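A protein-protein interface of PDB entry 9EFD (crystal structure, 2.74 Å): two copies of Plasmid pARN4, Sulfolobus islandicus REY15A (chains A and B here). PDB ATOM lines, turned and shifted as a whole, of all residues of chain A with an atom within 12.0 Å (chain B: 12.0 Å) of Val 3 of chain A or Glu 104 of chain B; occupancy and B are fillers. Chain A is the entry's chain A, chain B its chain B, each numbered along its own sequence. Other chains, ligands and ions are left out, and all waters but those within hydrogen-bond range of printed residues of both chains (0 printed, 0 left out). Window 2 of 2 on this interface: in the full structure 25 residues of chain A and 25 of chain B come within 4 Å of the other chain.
The backbone carbonyl oxygen (O) of Ile 94 of chain A lies within hydrogen-bond range of the backbone NH (N) of Ile 101 of chain B (2.7 Å). The backbone carbonyl oxygen (O) of Met 4 of chain A lies close to the backbone NH (N) of Glu 104 of chain B, 2.2 Å away. The backbone carbonyl oxygen of Val 102 of chain B is in hydrogen-bond range of the backbone NH of Val 6 of chain A, at 2.7 Å. The side-chain carboxylate (OD1) of Asp 103 of chain B sits close to the backbone carbonyl oxygen (O) of Met 4 of chain A. The backbone carbonyl oxygen (O) of Val 8 of chain A sits at hydrogen-bond distance from the backbone NH (N) of Tyr 100 of chain B, 2.5 Å away.
The backbone NH of Lys 105 of chain B sits at hydrogen-bond distance from the side-chain carboxylate of Asp 103 of chain B, 2.9 Å away. N of Ile 54 of chain A sits at hydrogen-bond distance from O of Ser 91 of chain A (2.7 Å). O of Ile 52 of chain A lies within hydrogen-bond range of N of Ile 93 of chain A, 2.7 Å away. NH2 of Arg 5 of chain A is in hydrogen-bond range of O of Thr 92 of chain A.
Among the printed residues, pairs that only touch across the chains: Val 3 of chain A with Glu 104 of chain B (3.9 Å), Met 4 of chain A with Val 102 of chain B (3.6 Å), Arg 5 of chain A with Ile 101 of chain B (3.8 Å), Arg 5 of chain A with Val 102 of chain B (3.2 Å), Arg 5 of chain A with Asp 103 of chain B (3.7 Å), Val 6 of chain A with Tyr 100 of chain B (3.5 Å), Val 6 of chain A with Ile 101 of chain B (3.4 Å), Val 6 of chain A with Leu 107 of chain B (3.7 Å), Lys 7 of chain A with Tyr 100 of chain B (3.3 Å), Val 8 of chain A with Val 102 of chain B (3.7 Å), Phe 13 of chain A with Tyr 100 of chain B (3.4 Å), Ile 16 of chain A with Ile 106 of chain B (3.8 Å), Ile 54 of chain A with Ile 106 of chain B (3.6 Å), Ser 91 of chain A with Asp 103 of chain B (3.97 Å), Ile 93 of chain A with Ile 101 of chain B (3.5 Å), Ile 93 of chain A with Val 102 of chain B (3.95 Å), Ile 93 of chain A with Ile 106 of chain B (3.99 Å) and Ile 94 of chain A with Tyr 100 of chain B (3.4 Å).
Of chain B, only Glu 104 comes within 4 Å of Val 3 of chain A. Of chain B, only Val 102 (3.6 Å), Asp 103 (2.9 Å) and Glu 104 (2.2 Å) come within 4 Å of Met 4 of chain A. Of chain B, only Tyr 100, Ile 101, Val 102 and Leu 107 come within 4 Å of Val 6 of chain A. Printed residues of chain B within 4 Å of Phe 13 of chain A: Tyr 100 (3.4 Å). Printed residues of chain B within 4 Å of Ile 16 of chain A: Ile 106 (3.8 Å). Met 23 of chain A touches none of the printed residues of chain B. Printed residues of chain B within 4 Å of Ile 54 of chain A: Ile 106 (3.6 Å). Pro 89 of chain A touches none of the printed residues of chain B. Of the printed residues of chain A, Ile 101 of chain B touches Arg 5, Val 6, Ile 93 and Ile 94. Asp 103 of chain B touches just these residues of chain A: Met 4, Arg 5 and Ser 91. Printed residues of chain A within 4 Å of Glu 104 of chain B: Val 3 (3.9 Å) and Met 4 (2.2 Å). Printed residues of chain A within 4 Å of Ile 106 of chain B: Ile 16 (3.8 Å), Ile 54 (3.6 Å) and Ile 93 (3.99 Å). Leu 107 of chain B touches just one residue of chain A: Val 6. No residue of chain A comes within 4 Å of Asp 109 of chain B. The nearest printed residue of chain B that does not touch Arg 5 of chain A is Glu 104 of chain B (4.4 Å).
Printed residues of chain A that touch a printed residue of chain B: Val 3, Met 4, Arg 5, Val 6, Lys 7, Val 8, Phe 13, Ile 16, Ile 54, Ser 91, Ile 93 and Ile 94. Printed residues of chain B that touch a printed residue of chain A: Tyr 100, Ile 101, Val 102, Asp 103, Glu 104, Ile 106 and Leu 107. Hydrophobic or aromatic side chains of chain B within 4 Å of the printed part of chain A: Tyr 100, Ile 101, Val 102, Ile 106 and Leu 107. Among the printed residues, no Asp or Glu carboxylate lies within 4 Å of a Lys or Arg side-chain nitrogen of the other chain.
No position is printed for both chains. Of the 23 pairs that touch across the chains among the printed residues, none has its exchanged pair printed and touching as well.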
ATOM      1  N   VAL A   3      11.652   6.292  27.861  1.00  0.00           N
ATOM      2  CA  VAL A   3      11.494   7.036  26.618  1.00  0.00           C
ATOM      3  C   VAL A   3      12.824   7.654  26.193  1.00  0.00           C
ATOM      4  O   VAL A   3      12.896   8.846  25.886  1.00  0.00           O
ATOM      5  CB  VAL A   3      10.403   8.120  26.755  1.00  0.00           C
ATOM      6  CG1 VAL A   3      10.813   9.171  27.781  1.00  0.00           C
ATOM      7  CG2 VAL A   3      10.111   8.761  25.405  1.00  0.00           C
ATOM      8  N   MET A   4      13.882   6.843  26.186  1.00  0.00           N
ATOM      9  CA  MET A   4      15.218   7.359  25.916  1.00  0.00           C
ATOM     10  C   MET A   4      15.523   7.396  24.427  1.00  0.00           C
ATOM     11  O   MET A   4      16.152   8.343  23.943  1.00  0.00           O
ATOM     12  CB  MET A   4      16.269   6.520  26.649  1.00  0.00           C
ATOM     13  CG  MET A   4      15.982   5.028  26.677  1.00  0.00           C
ATOM     14  SD  MET A   4      17.458   4.072  27.082  1.00  0.00           S
ATOM     15  CE  MET A   4      18.306   5.205  28.183  1.00  0.00           C
ATOM     16  N   ARG A   5      15.072   6.398  23.681  1.00  0.00           N
ATOM     17  CA  ARG A   5      15.456   6.240  22.285  1.00  0.00           C
ATOM     18  C   ARG A   5      14.297   6.622  21.375  1.00  0.00           C
ATOM     19  O   ARG A   5      13.217   6.027  21.446  1.00  0.00           O
ATOM     20  CB  ARG A   5      15.928   4.817  22.007  1.00  0.00           C
ATOM     21  CG  ARG A   5      16.962   4.368  23.012  1.00  0.00           C
ATOM     22  CD  ARG A   5      18.061   3.554  22.369  1.00  0.00           C
ATOM     23  NE  ARG A   5      19.253   4.358  22.127  1.00  0.00           N
ATOM     24  CZ  ARG A   5      20.019   4.230  21.052  1.00  0.00           C
ATOM     25  NH1 ARG A   5      19.879   3.203  20.229  1.00  0.00           N
ATOM     26  NH2 ARG A   5      20.954   5.146  20.805  1.00  0.00           N
ATOM     27  N   VAL A   6      14.537   7.606  20.512  1.00  0.00           N
ATOM     28  CA  VAL A   6      13.554   8.080  19.548  1.00  0.00           C
ATOM     29  C   VAL A   6      14.187   8.080  18.159  1.00  0.00           C
ATOM     30  O   VAL A   6      15.404   7.976  18.001  1.00  0.00           O
ATOM     31  CB  VAL A   6      13.015   9.486  19.894  1.00  0.00           C
ATOM     32  CG1 VAL A   6      12.634   9.574  21.367  1.00  0.00           C
ATOM     33  CG2 VAL A   6      14.037  10.553  19.539  1.00  0.00           C
ATOM     34  N   LYS A   7      13.338   8.196  17.144  1.00  0.00           N
ATOM     35  CA  LYS A   7      13.768   8.135  15.755  1.00  0.00           C
ATOM     36  C   LYS A   7      13.679   9.522  15.135  1.00  0.00           C
ATOM     37  O   LYS A   7      12.653  10.199  15.258  1.00  0.00           O
ATOM     38  CB  LYS A   7      12.922   7.139  14.960  1.00  0.00           C
ATOM     39  CG  LYS A   7      12.885   5.742  15.555  1.00  0.00           C
ATOM     40  CD  LYS A   7      12.179   4.763  14.630  1.00  0.00           C
ATOM     41  CE  LYS A   7      12.418   5.112  13.170  1.00  0.00           C
ATOM     42  NZ  LYS A   7      11.510   4.356  12.262  1.00  0.00           N
ATOM     43  N   VAL A   8      14.758   9.940  14.471  1.00  0.00           N
ATOM     44  CA  VAL A   8      14.817  11.227  13.793  1.00  0.00           C
ATOM     45  C   VAL A   8      15.300  11.008  12.364  1.00  0.00           C
ATOM     46  O   VAL A   8      15.925   9.996  12.040  1.00  0.00           O
ATOM     47  CB  VAL A   8      15.733  12.233  14.523  1.00  0.00           C
ATOM     48  CG1 VAL A   8      15.310  12.379  15.975  1.00  0.00           C
ATOM     49  CG2 VAL A   8      17.187  11.795  14.426  1.00  0.00           C
ATOM     50  N   GLN A  12      17.222  16.429  11.044  1.00  0.00           N
ATOM     51  CA  GLN A  12      17.456  16.564  12.478  1.00  0.00           C
ATOM     52  C   GLN A  12      18.796  15.963  12.884  1.00  0.00           C
ATOM     53  O   GLN A  12      19.533  16.557  13.682  1.00  0.00           O
ATOM     54  CB  GLN A  12      16.315  15.914  13.260  1.00  0.00           C
ATOM     55  CG  GLN A  12      15.031  15.755  12.463  1.00  0.00           C
ATOM     56  CD  GLN A  12      13.836  15.452  13.343  1.00  0.00           C
ATOM     57  OE1 GLN A  12      13.485  16.236  14.226  1.00  0.00           O
ATOM     58  NE2 GLN A  12      13.203  14.308  13.110  1.00  0.00           N
ATOM     59  N   PHE A  13      19.132  14.787  12.348  1.00  0.00           N
ATOM     60  CA  PHE A  13      20.421  14.179  12.658  1.00  0.00           C
ATOM     61  C   PHE A  13      21.572  15.047  12.170  1.00  0.00           C
ATOM     62  O   PHE A  13      22.582  15.206  12.866  1.00  0.00           O
ATOM     63  CB  PHE A  13      20.507  12.781  12.044  1.00  0.00           C
ATOM     64  CG  PHE A  13      21.898  12.216  12.018  1.00  0.00           C
ATOM     65  CD1 PHE A  13      22.463  11.677  13.162  1.00  0.00           C
ATOM     66  CD2 PHE A  13      22.642  12.225  10.849  1.00  0.00           C
ATOM     67  CE1 PHE A  13      23.743  11.156  13.142  1.00  0.00           C
ATOM     68  CE2 PHE A  13      23.923  11.706  10.823  1.00  0.00           C
ATOM     69  CZ  PHE A  13      24.474  11.170  11.970  1.00  0.00           C
ATOM     70  N   MET A  15      21.430  18.241  12.000  1.00  0.00           N
ATOM     71  CA  MET A  15      21.484  19.275  13.028  1.00  0.00           C
ATOM     72  C   MET A  15      22.221  18.783  14.266  1.00  0.00           C
ATOM     73  O   MET A  15      22.990  19.534  14.880  1.00  0.00           O
ATOM     74  CB  MET A  15      20.070  19.729  13.388  1.00  0.00           C
ATOM     75  CG  MET A  15      19.618  20.989  12.664  1.00  0.00           C
ATOM     76  SD  MET A  15      17.836  21.031  12.389  1.00  0.00           S
ATOM     77  CE  MET A  15      17.234  21.213  14.066  1.00  0.00           C
ATOM     78  N   ILE A  16      22.002  17.524  14.651  1.00  0.00           N
ATOM     79  CA  ILE A  16      22.685  16.973  15.819  1.00  0.00           C
ATOM     80  C   ILE A  16      24.194  16.992  15.608  1.00  0.00           C
ATOM     81  O   ILE A  16      24.957  17.416  16.484  1.00  0.00           O
ATOM     82  CB  ILE A  16      22.177  15.552  16.117  1.00  0.00           C
ATOM     83  CG1 ILE A  16      20.732  15.595  16.620  1.00  0.00           C
ATOM     84  CG2 ILE A  16      23.083  14.864  17.129  1.00  0.00           C
ATOM     85  CD1 ILE A  16      20.156  14.234  16.949  1.00  0.00           C
ATOM     86  N   LYS A  19      25.440  20.672  15.598  1.00  0.00           N
ATOM     87  CA  LYS A  19      25.559  21.231  16.941  1.00  0.00           C
ATOM     88  C   LYS A  19      26.854  20.786  17.609  1.00  0.00           C
ATOM     89  O   LYS A  19      27.545  21.592  18.241  1.00  0.00           O
ATOM     90  CB  LYS A  19      24.351  20.827  17.786  1.00  0.00           C
ATOM     91  CG  LYS A  19      23.030  21.402  17.303  1.00  0.00           C
ATOM     92  CD  LYS A  19      22.811  22.811  17.830  1.00  0.00           C
ATOM     93  CE  LYS A  19      21.631  23.482  17.144  1.00  0.00           C
ATOM     94  NZ  LYS A  19      21.446  22.998  15.748  1.00  0.00           N
ATOM     95  N   LEU A  20      27.199  19.502  17.480  1.00  0.00           N
ATOM     96  CA  LEU A  20      28.424  19.001  18.094  1.00  0.00           C
ATOM     97  C   LEU A  20      29.654  19.681  17.506  1.00  0.00           C
ATOM     98  O   LEU A  20      30.589  20.032  18.236  1.00  0.00           O
ATOM     99  CB  LEU A  20      28.516  17.485  17.923  1.00  0.00           C
ATOM    100  CG  LEU A  20      27.441  16.660  18.632  1.00  0.00           C
ATOM    101  CD1 LEU A  20      27.452  15.222  18.135  1.00  0.00           C
ATOM    102  CD2 LEU A  20      27.632  16.714  20.140  1.00  0.00           C
ATOM    103  N   MET A  23      30.160  22.826  18.955  1.00  0.00           N
ATOM    104  CA  MET A  23      30.562  22.695  20.351  1.00  0.00           C
ATOM    105  C   MET A  23      32.077  22.666  20.497  1.00  0.00           C
ATOM    106  O   MET A  23      32.611  23.148  21.502  1.00  0.00           O
ATOM    107  CB  MET A  23      29.946  21.436  20.962  1.00  0.00           C
ATOM    108  CG  MET A  23      29.376  21.639  22.352  1.00  0.00           C
ATOM    109  SD  MET A  23      28.163  20.382  22.796  1.00  0.00           S
ATOM    110  CE  MET A  23      26.719  21.404  23.086  1.00  0.00           C
ATOM    111  N   ILE A  52      27.095   5.965  14.814  1.00  0.00           N
ATOM    112  CA  ILE A  52      27.731   7.227  15.177  1.00  0.00           C
ATOM    113  C   ILE A  52      27.755   7.291  16.699  1.00  0.00           C
ATOM    114  O   ILE A  52      26.722   7.530  17.335  1.00  0.00           O
ATOM    115  CB  ILE A  52      27.006   8.441  14.586  1.00  0.00           C
ATOM    116  CG1 ILE A  52      26.782   8.245  13.086  1.00  0.00           C
ATOM    117  CG2 ILE A  52      27.800   9.711  14.847  1.00  0.00           C
ATOM    118  CD1 ILE A  52      25.419   7.686  12.741  1.00  0.00           C
ATOM    119  N   ILE A  54      28.871   9.341  19.987  1.00  0.00           N
ATOM    120  CA  ILE A  54      29.158  10.705  20.414  1.00  0.00           C
ATOM    121  C   ILE A  54      30.109  10.652  21.600  1.00  0.00           C
ATOM    122  O   ILE A  54      29.825   9.988  22.605  1.00  0.00           O
ATOM    123  CB  ILE A  54      27.869  11.461  20.774  1.00  0.00           C
ATOM    124  CG1 ILE A  54      26.802  11.250  19.697  1.00  0.00           C
ATOM    125  CG2 ILE A  54      28.156  12.943  20.960  1.00  0.00           C
ATOM    126  CD1 ILE A  54      27.259  11.621  18.302  1.00  0.00           C
ATOM    127  N   PRO A  89      28.714  14.924  25.753  1.00  0.00           N
ATOM    128  CA  PRO A  89      28.070  13.708  26.260  1.00  0.00           C
ATOM    129  C   PRO A  89      28.521  12.478  25.488  1.00  0.00           C
ATOM    130  O   PRO A  89      28.898  12.553  24.316  1.00  0.00           O
ATOM    131  CB  PRO A  89      26.577  13.983  26.053  1.00  0.00           C
ATOM    132  CG  PRO A  89      26.529  14.984  24.946  1.00  0.00           C
ATOM    133  CD  PRO A  89      27.756  15.836  25.105  1.00  0.00           C
ATOM    134  N   GLU A  90      28.483  11.333  26.164  1.00  0.00           N
ATOM    135  CA  GLU A  90      28.712  10.039  25.537  1.00  0.00           C
ATOM    136  C   GLU A  90      27.369   9.379  25.249  1.00  0.00           C
ATOM    137  O   GLU A  90      26.588   9.126  26.174  1.00  0.00           O
ATOM    138  CB  GLU A  90      29.572   9.146  26.433  1.00  0.00           C
ATOM    139  CG  GLU A  90      31.060   9.441  26.355  1.00  0.00           C
ATOM    140  CD  GLU A  90      31.891   8.193  26.133  1.00  0.00           C
ATOM    141  OE1 GLU A  90      31.523   7.128  26.672  1.00  0.00           O
ATOM    142  OE2 GLU A  90      32.913   8.278  25.421  1.00  0.00           O
ATOM    143  N   SER A  91      27.105   9.104  23.975  1.00  0.00           N
ATOM    144  CA  SER A  91      25.847   8.493  23.570  1.00  0.00           C
ATOM    145  C   SER A  91      26.036   7.834  22.211  1.00  0.00           C
ATOM    146  O   SER A  91      27.007   8.102  21.500  1.00  0.00           O
ATOM    147  CB  SER A  91      24.712   9.520  23.519  1.00  0.00           C
ATOM    148  OG  SER A  91      23.680   9.098  22.645  1.00  0.00           O
ATOM    149  N   THR A  92      25.091   6.964  21.864  1.00  0.00           N
ATOM    150  CA  THR A  92      25.166   6.157  20.653  1.00  0.00           C
ATOM    151  C   THR A  92      24.009   6.520  19.734  1.00  0.00           C
ATOM    152  O   THR A  92      22.848   6.511  20.156  1.00  0.00           O
ATOM    153  CB  THR A  92      25.131   4.660  20.978  1.00  0.00           C
ATOM    154  OG1 THR A  92      26.370   4.271  21.585  1.00  0.00           O
ATOM    155  CG2 THR A  92      24.915   3.846  19.711  1.00  0.00           C
ATOM    156  N   ILE A  93      24.329   6.833  18.481  1.00  0.00           N
ATOM    157  CA  ILE A  93      23.340   7.024  17.427  1.00  0.00           C
ATOM    158  C   ILE A  93      23.469   5.877  16.436  1.00  0.00           C
ATOM    159  O   ILE A  93      24.571   5.587  15.952  1.00  0.00           O
ATOM    160  CB  ILE A  93      23.517   8.379  16.721  1.00  0.00           C
ATOM    161  CG1 ILE A  93      23.154   9.527  17.666  1.00  0.00           C
ATOM    162  CG2 ILE A  93      22.673   8.435  15.458  1.00  0.00           C
ATOM    163  CD1 ILE A  93      23.247  10.895  17.025  1.00  0.00           C
ATOM    164  N   ILE A  94      22.349   5.230  16.133  1.00  0.00           N
ATOM    165  CA  ILE A  94      22.295   4.136  15.169  1.00  0.00           C
ATOM    166  C   ILE A  94      21.476   4.603  13.975  1.00  0.00           C
ATOM    167  O   ILE A  94      20.326   5.030  14.129  1.00  0.00           O
ATOM    168  CB  ILE A  94      21.696   2.865  15.787  1.00  0.00           C
ATOM    169  CG1 ILE A  94      22.553   2.387  16.960  1.00  0.00           C
ATOM    170  CG2 ILE A  94      21.566   1.773  14.735  1.00  0.00           C
ATOM    171  CD1 ILE A  94      21.810   1.506  17.938  1.00  0.00           C
ATOM    172  N   TYR B 100      17.306   7.853  12.015  1.00  0.00           N
ATOM    173  CA  TYR B 100      18.344   7.544  12.989  1.00  0.00           C
ATOM    174  C   TYR B 100      17.696   7.326  14.347  1.00  0.00           C
ATOM    175  O   TYR B 100      16.882   8.145  14.788  1.00  0.00           O
ATOM    176  CB  TYR B 100      19.383   8.667  13.069  1.00  0.00           C
ATOM    177  CG  TYR B 100      20.103   8.926  11.766  1.00  0.00           C
ATOM    178  CD1 TYR B 100      19.495   9.644  10.744  1.00  0.00           C
ATOM    179  CD2 TYR B 100      21.393   8.458  11.558  1.00  0.00           C
ATOM    180  CE1 TYR B 100      20.150   9.885   9.553  1.00  0.00           C
ATOM    181  CE2 TYR B 100      22.056   8.693  10.369  1.00  0.00           C
ATOM    182  CZ  TYR B 100      21.431   9.408   9.371  1.00  0.00           C
ATOM    183  OH  TYR B 100      22.090   9.645   8.186  1.00  0.00           O
ATOM    184  N   ILE B 101      18.058   6.229  15.005  1.00  0.00           N
ATOM    185  CA  ILE B 101      17.687   6.015  16.399  1.00  0.00           C
ATOM    186  C   ILE B 101      18.680   6.756  17.284  1.00  0.00           C
ATOM    187  O   ILE B 101      19.873   6.435  17.304  1.00  0.00           O
ATOM    188  CB  ILE B 101      17.649   4.519  16.742  1.00  0.00           C
ATOM    189  CG1 ILE B 101      16.928   3.738  15.641  1.00  0.00           C
ATOM    190  CG2 ILE B 101      16.965   4.301  18.085  1.00  0.00           C
ATOM    191  CD1 ILE B 101      16.981   2.236  15.822  1.00  0.00           C
ATOM    192  N   VAL B 102      18.189   7.747  18.017  1.00  0.00           N
ATOM    193  CA  VAL B 102      19.006   8.515  18.942  1.00  0.00           C
ATOM    194  C   VAL B 102      18.424   8.357  20.338  1.00  0.00           C
ATOM    195  O   VAL B 102      17.214   8.178  20.510  1.00  0.00           O
ATOM    196  CB  VAL B 102      19.086  10.006  18.538  1.00  0.00           C
ATOM    197  CG1 VAL B 102      19.299  10.131  17.038  1.00  0.00           C
ATOM    198  CG2 VAL B 102      17.824  10.752  18.964  1.00  0.00           C
ATOM    199  N   ASP B 103      19.298   8.420  21.339  1.00  0.00           N
ATOM    200  CA  ASP B 103      18.836   8.625  22.700  1.00  0.00           C
ATOM    201  C   ASP B 103      18.361  10.056  22.848  1.00  0.00           C
ATOM    202  O   ASP B 103      18.980  10.991  22.326  1.00  0.00           O
ATOM    203  CB  ASP B 103      19.936   8.334  23.725  1.00  0.00           C
ATOM    204  CG  ASP B 103      19.448   8.455  25.175  1.00  0.00           C
ATOM    205  OD1 ASP B 103      18.502   9.224  25.463  1.00  0.00           O
ATOM    206  OD2 ASP B 103      20.022   7.764  26.039  1.00  0.00           O
ATOM    207  N   GLU B 104      17.261  10.223  23.578  1.00  0.00           N
ATOM    208  CA  GLU B 104      16.667  11.542  23.682  1.00  0.00           C
ATOM    209  C   GLU B 104      17.588  12.541  24.359  1.00  0.00           C
ATOM    210  O   GLU B 104      17.638  13.699  23.929  1.00  0.00           O
ATOM    211  CB  GLU B 104      15.327  11.439  24.402  1.00  0.00           C
ATOM    212  CG  GLU B 104      14.385  12.513  23.964  1.00  0.00           C
ATOM    213  CD  GLU B 104      14.507  13.716  24.842  1.00  0.00           C
ATOM    214  OE1 GLU B 104      15.439  13.758  25.662  1.00  0.00           O
ATOM    215  OE2 GLU B 104      13.672  14.624  24.716  1.00  0.00           O
ATOM    216  N   LYS B 105      18.348  12.119  25.368  1.00  0.00           N
ATOM    217  CA  LYS B 105      19.125  13.081  26.137  1.00  0.00           C
ATOM    218  C   LYS B 105      19.996  13.934  25.227  1.00  0.00           C
ATOM    219  O   LYS B 105      20.241  15.108  25.522  1.00  0.00           O
ATOM    220  CB  LYS B 105      19.983  12.349  27.165  1.00  0.00           C
ATOM    221  N   ILE B 106      20.465  13.366  24.113  1.00  0.00           N
ATOM    222  CA  ILE B 106      21.242  14.145  23.152  1.00  0.00           C
ATOM    223  C   ILE B 106      20.396  15.264  22.552  1.00  0.00           C
ATOM    224  O   ILE B 106      20.867  16.396  22.387  1.00  0.00           O
ATOM    225  CB  ILE B 106      21.832  13.225  22.065  1.00  0.00           C
ATOM    226  CG1 ILE B 106      22.977  13.932  21.335  1.00  0.00           C
ATOM    227  CG2 ILE B 106      20.763  12.790  21.073  1.00  0.00           C
ATOM    228  CD1 ILE B 106      23.721  13.047  20.357  1.00  0.00           C
ATOM    229  N   LEU B 107      19.138  14.969  22.208  1.00  0.00           N
ATOM    230  CA  LEU B 107      18.208  16.029  21.832  1.00  0.00           C
ATOM    231  C   LEU B 107      17.967  16.985  22.992  1.00  0.00           C
ATOM    232  O   LEU B 107      17.960  18.208  22.811  1.00  0.00           O
ATOM    233  CB  LEU B 107      16.886  15.424  21.358  1.00  0.00           C
ATOM    234  CG  LEU B 107      16.891  14.764  19.979  1.00  0.00           C
ATOM    235  CD1 LEU B 107      15.730  13.789  19.838  1.00  0.00           C
ATOM    236  CD2 LEU B 107      16.851  15.812  18.879  1.00  0.00           C
ATOM    237  N   TYR B 108      17.769  16.443  24.195  1.00  0.00           N
ATOM    238  CA  TYR B 108      17.702  17.279  25.387  1.00  0.00           C
ATOM    239  C   TYR B 108      19.016  18.007  25.629  1.00  0.00           C
ATOM    240  O   TYR B 108      19.025  19.090  26.226  1.00  0.00           O
ATOM    241  CB  TYR B 108      17.306  16.416  26.592  1.00  0.00           C
ATOM    242  CG  TYR B 108      17.486  17.043  27.964  1.00  0.00           C
ATOM    243  CD1 TYR B 108      18.748  17.209  28.525  1.00  0.00           C
ATOM    244  CD2 TYR B 108      16.385  17.465  28.699  1.00  0.00           C
ATOM    245  CE1 TYR B 108      18.906  17.776  29.776  1.00  0.00           C
ATOM    246  CE2 TYR B 108      16.535  18.035  29.949  1.00  0.00           C
ATOM    247  CZ  TYR B 108      17.797  18.189  30.483  1.00  0.00           C
ATOM    248  OH  TYR B 108      17.948  18.755  31.728  1.00  0.00           O
ATOM    249  N   ASP B 109      20.129  17.443  25.168  1.00  0.00           N
ATOM    250  CA  ASP B 109      21.457  17.907  25.558  1.00  0.00           C
ATOM    251  C   ASP B 109      21.688  17.704  27.053  1.00  0.00           C
ATOM    252  O   ASP B 109      21.897  16.579  27.509  1.00  0.00           O
ATOM    253  CB  ASP B 109      21.647  19.381  25.186  1.00  0.00           C
ATOM    254  CG  ASP B 109      21.194  19.688  23.771  1.00  0.00           C
ATOM    255  OD1 ASP B 109      21.968  19.421  22.827  1.00  0.00           O
ATOM    256  OD2 ASP B 109      20.062  20.188  23.601  1.00  0.00           O
